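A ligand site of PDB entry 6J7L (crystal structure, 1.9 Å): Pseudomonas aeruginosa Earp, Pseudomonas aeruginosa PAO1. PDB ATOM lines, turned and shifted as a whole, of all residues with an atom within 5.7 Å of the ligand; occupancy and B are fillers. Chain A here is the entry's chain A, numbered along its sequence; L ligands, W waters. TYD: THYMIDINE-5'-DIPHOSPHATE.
CB of Asn 32 touches O2B of the ligand (3.3 Å).
Gly 37 touches the ligand.
Ile 67 touches the ligand.
CD1 of Phe 209 touches C5M of the ligand (3.6 Å).
CB of Pro 235 touches C5M of the ligand, 3.9 Å away.
CE2 of Phe 270 touches C5 of the ligand, 3.4 Å away.
C of Ala 272 touches O2 of the ligand, 3.9 Å away.
Tyr 276 touches the ligand.
CA of Gly 290 touches O3A of the ligand (3.5 Å).
Hydrophobic or aromatic side chains that line the ligand: Tyr 33, Ile 67, Phe 209, Tyr 211, Pro 235, Phe 270, Met 271 and Tyr 276.
18 residues have an atom within 4 Å of the ligand: Asn 32, Tyr 33, Gly 34, Gly 37, Ile 67, Phe 209, Tyr 211, Pro 235, Phe 270, Met 271, Ala 272, Gln 273, Tyr 276, Arg 289, Gly 290, Glu 291, Asp 292 and Ser 293.
Along chain A the residues within 4 Å of the ligand span positions 32 to 293.
O of Met 271 sits at hydrogen-bond distance from N3 of the ligand (2.6 Å).
The backbone NH of Gly 34 lies within hydrogen-bond range of an oxygen (O3B) of the ligand (2.9 Å).
The backbone NH of Met 271 is in hydrogen-bond range of an oxygen (O4) of the ligand, 3.1 Å away.
The side-chain hydroxyl (OG) of Ser 293 is in hydrogen-bond range of an oxygen (O1A) of the ligand, 2.7 Å away.
NE of Arg 289 lies within salt-bridge range of O1B of the ligand, at 2.8 Å.
An oxygen (O3') of the ligand lies within hydrogen-bond range of the side-chain amide nitrogen of Gln 273 (3.1 Å).
An oxygen (O2A) of the ligand sits at hydrogen-bond distance from the backbone NH (N) of Asp 292, 2.7 Å away.
N of Tyr 33 sits at hydrogen-bond distance from O2B of the ligand, at 2.9 Å.
An oxygen (O3') of the ligand is in hydrogen-bond range of the side-chain carboxylate (OD2) of Asp 292 (2.6 Å).
The backbone NH (N) of Glu 291 lies within hydrogen-bond range of an oxygen (O2A) of the ligand (2.7 Å).
The backbone NH (N) of Ser 293 lies within hydrogen-bond range of an oxygen (O1A) of the ligand, 2.7 Å away.
O1B of the ligand is in hydrogen-bond range of OH of Tyr 211 (2.5 Å).
O of Arg 289 sits at hydrogen-bond distance from N of Phe 294 (3.4 Å).
The side-chain hydroxyl (OG) of Ser 293 lies within hydrogen-bond range of the backbone carbonyl oxygen (O) of Arg 289 (2.7 Å).
O of Ile 67 sits at hydrogen-bond distance from N of Gln 273.
The backbone NH (N) of Gly 290 lies within hydrogen-bond range of the side-chain hydroxyl (OH) of Tyr 211.
The backbone carbonyl oxygen (O) of Gly 37 is in hydrogen-bond range of the side-chain amide nitrogen (NE2) of Gln 273, 3.0 Å away.
OD1 of Asp 292 is in salt-bridge range of NE of Arg 41 (2.8 Å).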
ATOM      1  N   ASP A  31      25.229 -11.458   7.672  1.00  0.00           N
ATOM      2  CA  ASP A  31      25.335 -11.213   6.237  1.00  0.00           C
ATOM      3  C   ASP A  31      23.938 -11.098   5.665  1.00  0.00           C
ATOM      4  O   ASP A  31      22.980 -11.663   6.203  1.00  0.00           O
ATOM      5  CB  ASP A  31      26.110 -12.329   5.526  1.00  0.00           C
ATOM      6  CG  ASP A  31      27.614 -12.159   5.628  1.00  0.00           C
ATOM      7  OD1 ASP A  31      28.091 -11.007   5.510  1.00  0.00           O
ATOM      8  OD2 ASP A  31      28.319 -13.167   5.819  1.00  0.00           O
ATOM      9  N   ASN A  32      23.829 -10.353   4.564  1.00  0.00           N
ATOM     10  CA  ASN A  32      22.577 -10.212   3.818  1.00  0.00           C
ATOM     11  C   ASN A  32      21.481  -9.578   4.677  1.00  0.00           C
ATOM     12  O   ASN A  32      21.775  -8.951   5.698  1.00  0.00           O
ATOM     13  CB  ASN A  32      22.145 -11.571   3.268  1.00  0.00           C
ATOM     14  CG  ASN A  32      23.237 -12.236   2.446  1.00  0.00           C
ATOM     15  OD1 ASN A  32      23.896 -11.585   1.640  1.00  0.00           O
ATOM     16  ND2 ASN A  32      23.456 -13.529   2.665  1.00  0.00           N
ATOM     17  N   TYR A  33      20.223  -9.742   4.272  1.00  0.00           N
ATOM     18  CA  TYR A  33      19.159  -8.905   4.814  1.00  0.00           C
ATOM     19  C   TYR A  33      18.027  -9.647   5.501  1.00  0.00           C
ATOM     20  O   TYR A  33      17.205  -8.998   6.146  1.00  0.00           O
ATOM     21  CB  TYR A  33      18.551  -8.038   3.692  1.00  0.00           C
ATOM     22  CG  TYR A  33      19.524  -7.083   3.035  1.00  0.00           C
ATOM     23  CD1 TYR A  33      20.090  -7.373   1.804  1.00  0.00           C
ATOM     24  CD2 TYR A  33      19.883  -5.885   3.657  1.00  0.00           C
ATOM     25  CE1 TYR A  33      20.975  -6.494   1.188  1.00  0.00           C
ATOM     26  CE2 TYR A  33      20.765  -5.009   3.054  1.00  0.00           C
ATOM     27  CZ  TYR A  33      21.317  -5.315   1.824  1.00  0.00           C
ATOM     28  OH  TYR A  33      22.188  -4.434   1.234  1.00  0.00           O
ATOM     29  N   GLY A  34      17.962 -10.975   5.396  1.00  0.00           N
ATOM     30  CA  GLY A  34      16.791 -11.686   5.887  1.00  0.00           C
ATOM     31  C   GLY A  34      16.709 -11.797   7.381  1.00  0.00           C
ATOM     32  O   GLY A  34      15.604 -11.961   7.919  1.00  0.00           O
ATOM     33  N   ASP A  35      17.842 -11.702   8.076  1.00  0.00           N
ATOM     34  CA  ASP A  35      17.736 -11.768   9.535  1.00  0.00           C
ATOM     35  C   ASP A  35      17.102 -10.500  10.063  1.00  0.00           C
ATOM     36  O   ASP A  35      16.201 -10.556  10.896  1.00  0.00           O
ATOM     37  CB  ASP A  35      19.112 -12.051  10.153  1.00  0.00           C
ATOM     38  CG  ASP A  35      19.541 -13.503   9.936  1.00  0.00           C
ATOM     39  OD1 ASP A  35      18.880 -14.214   9.145  1.00  0.00           O
ATOM     40  OD2 ASP A  35      20.527 -13.941  10.559  1.00  0.00           O
ATOM     41  N   GLY A  37      15.327  -8.633   8.006  1.00  0.00           N
ATOM     42  CA  GLY A  37      14.047  -8.620   7.325  1.00  0.00           C
ATOM     43  C   GLY A  37      12.977  -9.361   8.115  1.00  0.00           C
ATOM     44  O   GLY A  37      11.865  -8.853   8.292  1.00  0.00           O
ATOM     45  N   VAL A  38      13.310 -10.556   8.606  1.00  0.00           N
ATOM     46  CA  VAL A  38      12.344 -11.364   9.357  1.00  0.00           C
ATOM     47  C   VAL A  38      12.030 -10.735  10.708  1.00  0.00           C
ATOM     48  O   VAL A  38      10.865 -10.679  11.123  1.00  0.00           O
ATOM     49  CB  VAL A  38      12.855 -12.816   9.534  1.00  0.00           C
ATOM     50  CG1 VAL A  38      12.053 -13.558  10.600  1.00  0.00           C
ATOM     51  CG2 VAL A  38      12.796 -13.581   8.197  1.00  0.00           C
ATOM     52  N   ARG A  41       9.881  -7.627  10.199  1.00  0.00           N
ATOM     53  CA  ARG A  41       8.513  -8.021   9.875  1.00  0.00           C
ATOM     54  C   ARG A  41       7.750  -8.442  11.118  1.00  0.00           C
ATOM     55  O   ARG A  41       6.605  -8.011  11.340  1.00  0.00           O
ATOM     56  CB  ARG A  41       8.529  -9.181   8.869  1.00  0.00           C
ATOM     57  CG  ARG A  41       7.136  -9.555   8.373  1.00  0.00           C
ATOM     58  CD  ARG A  41       7.191 -10.651   7.269  1.00  0.00           C
ATOM     59  NE  ARG A  41       7.998 -10.249   6.122  1.00  0.00           N
ATOM     60  CZ  ARG A  41       7.679  -9.303   5.244  1.00  0.00           C
ATOM     61  NH1 ARG A  41       6.551  -8.581   5.367  1.00  0.00           N
ATOM     62  NH2 ARG A  41       8.502  -9.036   4.230  1.00  0.00           N
ATOM     63  N   ARG A  66      18.382  -0.343   4.767  1.00  0.00           N
ATOM     64  CA  ARG A  66      18.158  -0.845   3.416  1.00  0.00           C
ATOM     65  C   ARG A  66      16.719  -1.349   3.233  1.00  0.00           C
ATOM     66  O   ARG A  66      16.049  -0.980   2.258  1.00  0.00           O
ATOM     67  CB  ARG A  66      19.155  -1.958   3.097  1.00  0.00           C
ATOM     68  N   ILE A  67      16.228  -2.162   4.167  1.00  0.00           N
ATOM     69  CA  ILE A  67      14.880  -2.712   4.019  1.00  0.00           C
ATOM     70  C   ILE A  67      13.799  -1.752   4.491  1.00  0.00           C
ATOM     71  O   ILE A  67      12.610  -1.981   4.194  1.00  0.00           O
ATOM     72  CB  ILE A  67      14.722  -4.047   4.783  1.00  0.00           C
ATOM     73  CG1 ILE A  67      15.049  -3.867   6.263  1.00  0.00           C
ATOM     74  CG2 ILE A  67      15.610  -5.123   4.165  1.00  0.00           C
ATOM     75  CD1 ILE A  67      14.531  -5.008   7.132  1.00  0.00           C
ATOM     76  N   PHE A 209      16.241 -12.442  -7.577  1.00  0.00           N
ATOM     77  CA  PHE A 209      16.870 -12.084  -6.312  1.00  0.00           C
ATOM     78  C   PHE A 209      17.606 -13.334  -5.876  1.00  0.00           C
ATOM     79  O   PHE A 209      16.988 -14.341  -5.522  1.00  0.00           O
ATOM     80  CB  PHE A 209      15.792 -11.654  -5.301  1.00  0.00           C
ATOM     81  CG  PHE A 209      16.317 -11.255  -3.950  1.00  0.00           C
ATOM     82  CD1 PHE A 209      17.331 -10.316  -3.825  1.00  0.00           C
ATOM     83  CD2 PHE A 209      15.734 -11.768  -2.784  1.00  0.00           C
ATOM     84  CE1 PHE A 209      17.804  -9.935  -2.563  1.00  0.00           C
ATOM     85  CE2 PHE A 209      16.193 -11.387  -1.518  1.00  0.00           C
ATOM     86  CZ  PHE A 209      17.226 -10.471  -1.401  1.00  0.00           C
ATOM     87  N   TYR A 211      21.811 -15.239  -4.923  1.00  0.00           N
ATOM     88  CA  TYR A 211      23.214 -15.031  -4.632  1.00  0.00           C
ATOM     89  C   TYR A 211      23.983 -15.226  -5.939  1.00  0.00           C
ATOM     90  O   TYR A 211      23.398 -15.491  -6.985  1.00  0.00           O
ATOM     91  CB  TYR A 211      23.709 -15.977  -3.528  1.00  0.00           C
ATOM     92  CG  TYR A 211      22.820 -16.006  -2.311  1.00  0.00           C
ATOM     93  CD1 TYR A 211      21.999 -17.092  -2.048  1.00  0.00           C
ATOM     94  CD2 TYR A 211      22.789 -14.931  -1.434  1.00  0.00           C
ATOM     95  CE1 TYR A 211      21.152 -17.098  -0.935  1.00  0.00           C
ATOM     96  CE2 TYR A 211      21.954 -14.925  -0.331  1.00  0.00           C
ATOM     97  CZ  TYR A 211      21.152 -16.005  -0.077  1.00  0.00           C
ATOM     98  OH  TYR A 211      20.328 -16.002   1.035  1.00  0.00           O
ATOM     99  N   PRO A 235      16.385  -6.422  -9.064  1.00  0.00           N
ATOM    100  CA  PRO A 235      16.733  -5.440  -8.011  1.00  0.00           C
ATOM    101  C   PRO A 235      18.230  -5.458  -7.768  1.00  0.00           C
ATOM    102  O   PRO A 235      18.857  -6.521  -7.789  1.00  0.00           O
ATOM    103  CB  PRO A 235      15.962  -5.945  -6.785  1.00  0.00           C
ATOM    104  CG  PRO A 235      14.908  -6.913  -7.308  1.00  0.00           C
ATOM    105  CD  PRO A 235      15.522  -7.505  -8.559  1.00  0.00           C
ATOM    106  N   PRO A 269      15.647  -0.571  -8.531  1.00  0.00           N
ATOM    107  CA  PRO A 269      16.227  -0.190  -7.237  1.00  0.00           C
ATOM    108  C   PRO A 269      15.925  -1.247  -6.192  1.00  0.00           C
ATOM    109  O   PRO A 269      14.977  -2.028  -6.317  1.00  0.00           O
ATOM    110  CB  PRO A 269      15.541   1.141  -6.902  1.00  0.00           C
ATOM    111  CG  PRO A 269      14.231   1.074  -7.641  1.00  0.00           C
ATOM    112  CD  PRO A 269      14.492   0.278  -8.901  1.00  0.00           C
ATOM    113  N   PHE A 270      16.752  -1.281  -5.142  1.00  0.00           N
ATOM    114  CA  PHE A 270      16.446  -2.082  -3.956  1.00  0.00           C
ATOM    115  C   PHE A 270      15.378  -1.307  -3.190  1.00  0.00           C
ATOM    116  O   PHE A 270      15.639  -0.196  -2.703  1.00  0.00           O
ATOM    117  CB  PHE A 270      17.688  -2.329  -3.091  1.00  0.00           C
ATOM    118  CG  PHE A 270      17.491  -3.359  -2.001  1.00  0.00           C
ATOM    119  CD1 PHE A 270      17.002  -2.999  -0.747  1.00  0.00           C
ATOM    120  CD2 PHE A 270      17.790  -4.702  -2.223  1.00  0.00           C
ATOM    121  CE1 PHE A 270      16.798  -3.953   0.266  1.00  0.00           C
ATOM    122  CE2 PHE A 270      17.604  -5.667  -1.222  1.00  0.00           C
ATOM    123  CZ  PHE A 270      17.112  -5.281   0.022  1.00  0.00           C
ATOM    124  N   MET A 271      14.181  -1.870  -3.121  1.00  0.00           N
ATOM    125  CA  MET A 271      12.984  -1.170  -2.679  1.00  0.00           C
ATOM    126  C   MET A 271      12.572  -1.584  -1.272  1.00  0.00           C
ATOM    127  O   MET A 271      13.096  -2.537  -0.700  1.00  0.00           O
ATOM    128  CB  MET A 271      11.838  -1.417  -3.669  1.00  0.00           C
ATOM    129  CG  MET A 271      11.428  -2.883  -3.791  1.00  0.00           C
ATOM    130  SD  MET A 271      10.663  -3.310  -5.402  1.00  0.00           S
ATOM    131  CE  MET A 271      12.104  -3.769  -6.341  1.00  0.00           C
ATOM    132  N   ALA A 272      11.611  -0.842  -0.723  1.00  0.00           N
ATOM    133  CA  ALA A 272      11.087  -1.162   0.601  1.00  0.00           C
ATOM    134  C   ALA A 272      10.445  -2.546   0.602  1.00  0.00           C
ATOM    135  O   ALA A 272       9.971  -3.041  -0.415  1.00  0.00           O
ATOM    136  CB  ALA A 272      10.077  -0.098   1.048  1.00  0.00           C
ATOM    137  N   GLN A 273      10.438  -3.172   1.793  1.00  0.00           N
ATOM    138  CA  GLN A 273       9.917  -4.533   1.915  1.00  0.00           C
ATOM    139  C   GLN A 273       8.509  -4.679   1.324  1.00  0.00           C
ATOM    140  O   GLN A 273       8.222  -5.672   0.645  1.00  0.00           O
ATOM    141  CB  GLN A 273       9.889  -4.910   3.404  1.00  0.00           C
ATOM    142  CG  GLN A 273      10.578  -6.188   3.742  1.00  0.00           C
ATOM    143  CD  GLN A 273      10.554  -6.458   5.229  1.00  0.00           C
ATOM    144  OE1 GLN A 273       9.825  -5.805   5.979  1.00  0.00           O
ATOM    145  NE2 GLN A 273      11.351  -7.422   5.656  1.00  0.00           N
ATOM    146  N   TYR A 276       8.551  -4.626  -2.371  1.00  0.00           N
ATOM    147  CA  TYR A 276       9.044  -5.887  -2.923  1.00  0.00           C
ATOM    148  C   TYR A 276       7.928  -6.931  -2.980  1.00  0.00           C
ATOM    149  O   TYR A 276       7.849  -7.705  -3.940  1.00  0.00           O
ATOM    150  CB  TYR A 276      10.238  -6.380  -2.106  1.00  0.00           C
ATOM    151  CG  TYR A 276      10.847  -7.674  -2.614  1.00  0.00           C
ATOM    152  CD1 TYR A 276      11.432  -7.755  -3.863  1.00  0.00           C
ATOM    153  CD2 TYR A 276      10.826  -8.816  -1.820  1.00  0.00           C
ATOM    154  CE1 TYR A 276      11.987  -8.941  -4.320  1.00  0.00           C
ATOM    155  CE2 TYR A 276      11.377 -10.021  -2.268  1.00  0.00           C
ATOM    156  CZ  TYR A 276      11.957 -10.061  -3.510  1.00  0.00           C
ATOM    157  OH  TYR A 276      12.516 -11.243  -3.959  1.00  0.00           O
ATOM    158  N   ARG A 289      15.494 -15.934  -2.500  1.00  0.00           N
ATOM    159  CA  ARG A 289      16.572 -16.589  -1.790  1.00  0.00           C
ATOM    160  C   ARG A 289      16.281 -16.572  -0.292  1.00  0.00           C
ATOM    161  O   ARG A 289      15.217 -16.125   0.158  1.00  0.00           O
ATOM    162  CB  ARG A 289      17.890 -15.914  -2.098  1.00  0.00           C
ATOM    163  CG  ARG A 289      17.892 -14.497  -1.668  1.00  0.00           C
ATOM    164  CD  ARG A 289      19.152 -13.771  -2.048  1.00  0.00           C
ATOM    165  NE  ARG A 289      19.490 -12.788  -1.027  1.00  0.00           N
ATOM    166  CZ  ARG A 289      20.243 -11.715  -1.249  1.00  0.00           C
ATOM    167  NH1 ARG A 289      20.727 -11.473  -2.456  1.00  0.00           N
ATOM    168  NH2 ARG A 289      20.479 -10.871  -0.247  1.00  0.00           N
ATOM    169  N   GLY A 290      17.237 -17.091   0.480  1.00  0.00           N
ATOM    170  CA  GLY A 290      17.232 -16.873   1.918  1.00  0.00           C
ATOM    171  C   GLY A 290      15.983 -17.404   2.585  1.00  0.00           C
ATOM    172  O   GLY A 290      15.546 -18.540   2.339  1.00  0.00           O
ATOM    173  N   GLU A 291      15.384 -16.573   3.441  1.00  0.00           N
ATOM    174  CA  GLU A 291      14.249 -16.999   4.264  1.00  0.00           C
ATOM    175  C   GLU A 291      13.015 -16.134   4.086  1.00  0.00           C
ATOM    176  O   GLU A 291      11.914 -16.673   3.872  1.00  0.00           O
ATOM    177  CB  GLU A 291      14.642 -16.997   5.742  1.00  0.00           C
ATOM    178  CG  GLU A 291      13.486 -17.383   6.612  1.00  0.00           C
ATOM    179  CD  GLU A 291      13.940 -17.780   7.981  1.00  0.00           C
ATOM    180  OE1 GLU A 291      13.712 -17.014   8.934  1.00  0.00           O
ATOM    181  OE2 GLU A 291      14.570 -18.845   8.086  1.00  0.00           O
ATOM    182  N   ASP A 292      13.147 -14.807   4.191  1.00  0.00           N
ATOM    183  CA  ASP A 292      11.948 -13.955   4.122  1.00  0.00           C
ATOM    184  C   ASP A 292      11.383 -13.916   2.707  1.00  0.00           C
ATOM    185  O   ASP A 292      10.191 -14.156   2.496  1.00  0.00           O
ATOM    186  CB  ASP A 292      12.255 -12.543   4.622  1.00  0.00           C
ATOM    187  CG  ASP A 292      10.989 -11.676   4.739  1.00  0.00           C
ATOM    188  OD1 ASP A 292      10.103 -12.041   5.543  1.00  0.00           O
ATOM    189  OD2 ASP A 292      10.866 -10.670   4.020  1.00  0.00           O
ATOM    190  N   SER A 293      12.220 -13.589   1.708  1.00  0.00           N
ATOM    191  CA  SER A 293      11.696 -13.517   0.345  1.00  0.00           C
ATOM    192  C   SER A 293      11.166 -14.871  -0.094  1.00  0.00           C
ATOM    193  O   SER A 293      10.211 -14.940  -0.860  1.00  0.00           O
ATOM    194  CB  SER A 293      12.760 -13.033  -0.639  1.00  0.00           C
ATOM    195  OG  SER A 293      13.815 -13.980  -0.753  1.00  0.00           O
ATOM    196  N   PHE A 294      11.781 -15.937   0.405  1.00  0.00           N
ATOM    197  CA  PHE A 294      11.295 -17.292   0.123  1.00  0.00           C
ATOM    198  C   PHE A 294       9.824 -17.436   0.491  1.00  0.00           C
ATOM    199  O   PHE A 294       9.009 -17.902  -0.321  1.00  0.00           O
ATOM    200  CB  PHE A 294      12.177 -18.286   0.889  1.00  0.00           C
ATOM    201  CG  PHE A 294      11.755 -19.736   0.753  1.00  0.00           C
ATOM    202  CD1 PHE A 294      11.540 -20.295  -0.495  1.00  0.00           C
ATOM    203  CD2 PHE A 294      11.616 -20.525   1.877  1.00  0.00           C
ATOM    204  CE1 PHE A 294      11.179 -21.649  -0.614  1.00  0.00           C
ATOM    205  CE2 PHE A 294      11.256 -21.878   1.758  1.00  0.00           C
ATOM    206  CZ  PHE A 294      11.036 -22.426   0.518  1.00  0.00           C
HETATM  207  PA  TYD L   1      15.885 -12.962   2.581  1.00  0.00           P
HETATM  208  O1A TYD L   1      14.828 -13.075   1.525  1.00  0.00           O
HETATM  209  O2A TYD L   1      15.612 -13.861   3.764  1.00  0.00           O
HETATM  210  O3A TYD L   1      17.354 -13.399   1.954  1.00  0.00           O
HETATM  211  PB  TYD L   1      18.847 -12.873   2.441  1.00  0.00           P
HETATM  212  O1B TYD L   1      19.862 -13.651   1.604  1.00  0.00           O
HETATM  213  O2B TYD L   1      19.037 -11.407   2.180  1.00  0.00           O
HETATM  214  O3B TYD L   1      19.033 -13.168   3.914  1.00  0.00           O
HETATM  215  O5' TYD L   1      15.978 -11.402   3.043  1.00  0.00           O
HETATM  216  C5' TYD L   1      16.016 -10.393   1.993  1.00  0.00           C
HETATM  217  C4' TYD L   1      15.202  -9.214   2.530  1.00  0.00           C
HETATM  218  O4' TYD L   1      15.388  -8.186   1.776  1.00  0.00           O
HETATM  219  C3' TYD L   1      13.600  -9.589   2.471  1.00  0.00           C
HETATM  220  O3' TYD L   1      12.987  -9.156   3.747  1.00  0.00           O
HETATM  221  C2' TYD L   1      13.162  -8.973   1.469  1.00  0.00           C
HETATM  222  C1' TYD L   1      14.015  -7.659   1.439  1.00  0.00           C
HETATM  223  N1  TYD L   1      14.070  -7.011   0.233  1.00  0.00           N
HETATM  224  C2  TYD L   1      13.680  -5.713   0.196  1.00  0.00           C
HETATM  225  O2  TYD L   1      13.295  -5.169   1.220  1.00  0.00           O
HETATM  226  N3  TYD L   1      13.733  -5.007  -1.000  1.00  0.00           N
HETATM  227  C4  TYD L   1      14.154  -5.607  -2.114  1.00  0.00           C
HETATM  228  O4  TYD L   1      14.194  -4.992  -3.152  1.00  0.00           O
HETATM  229  C5  TYD L   1      14.556  -6.923  -2.085  1.00  0.00           C
HETATM  230  C5M TYD L   1      15.047  -7.595  -3.409  1.00  0.00           C
HETATM  231  C6  TYD L   1      14.503  -7.628  -0.889  1.00  0.00           C
HETATM  232  O   HOH W   1      18.108 -15.145   5.379  1.00  0.00           O
HETATM  233  O   HOH W   2      10.683 -10.395   1.218  1.00  0.00           O
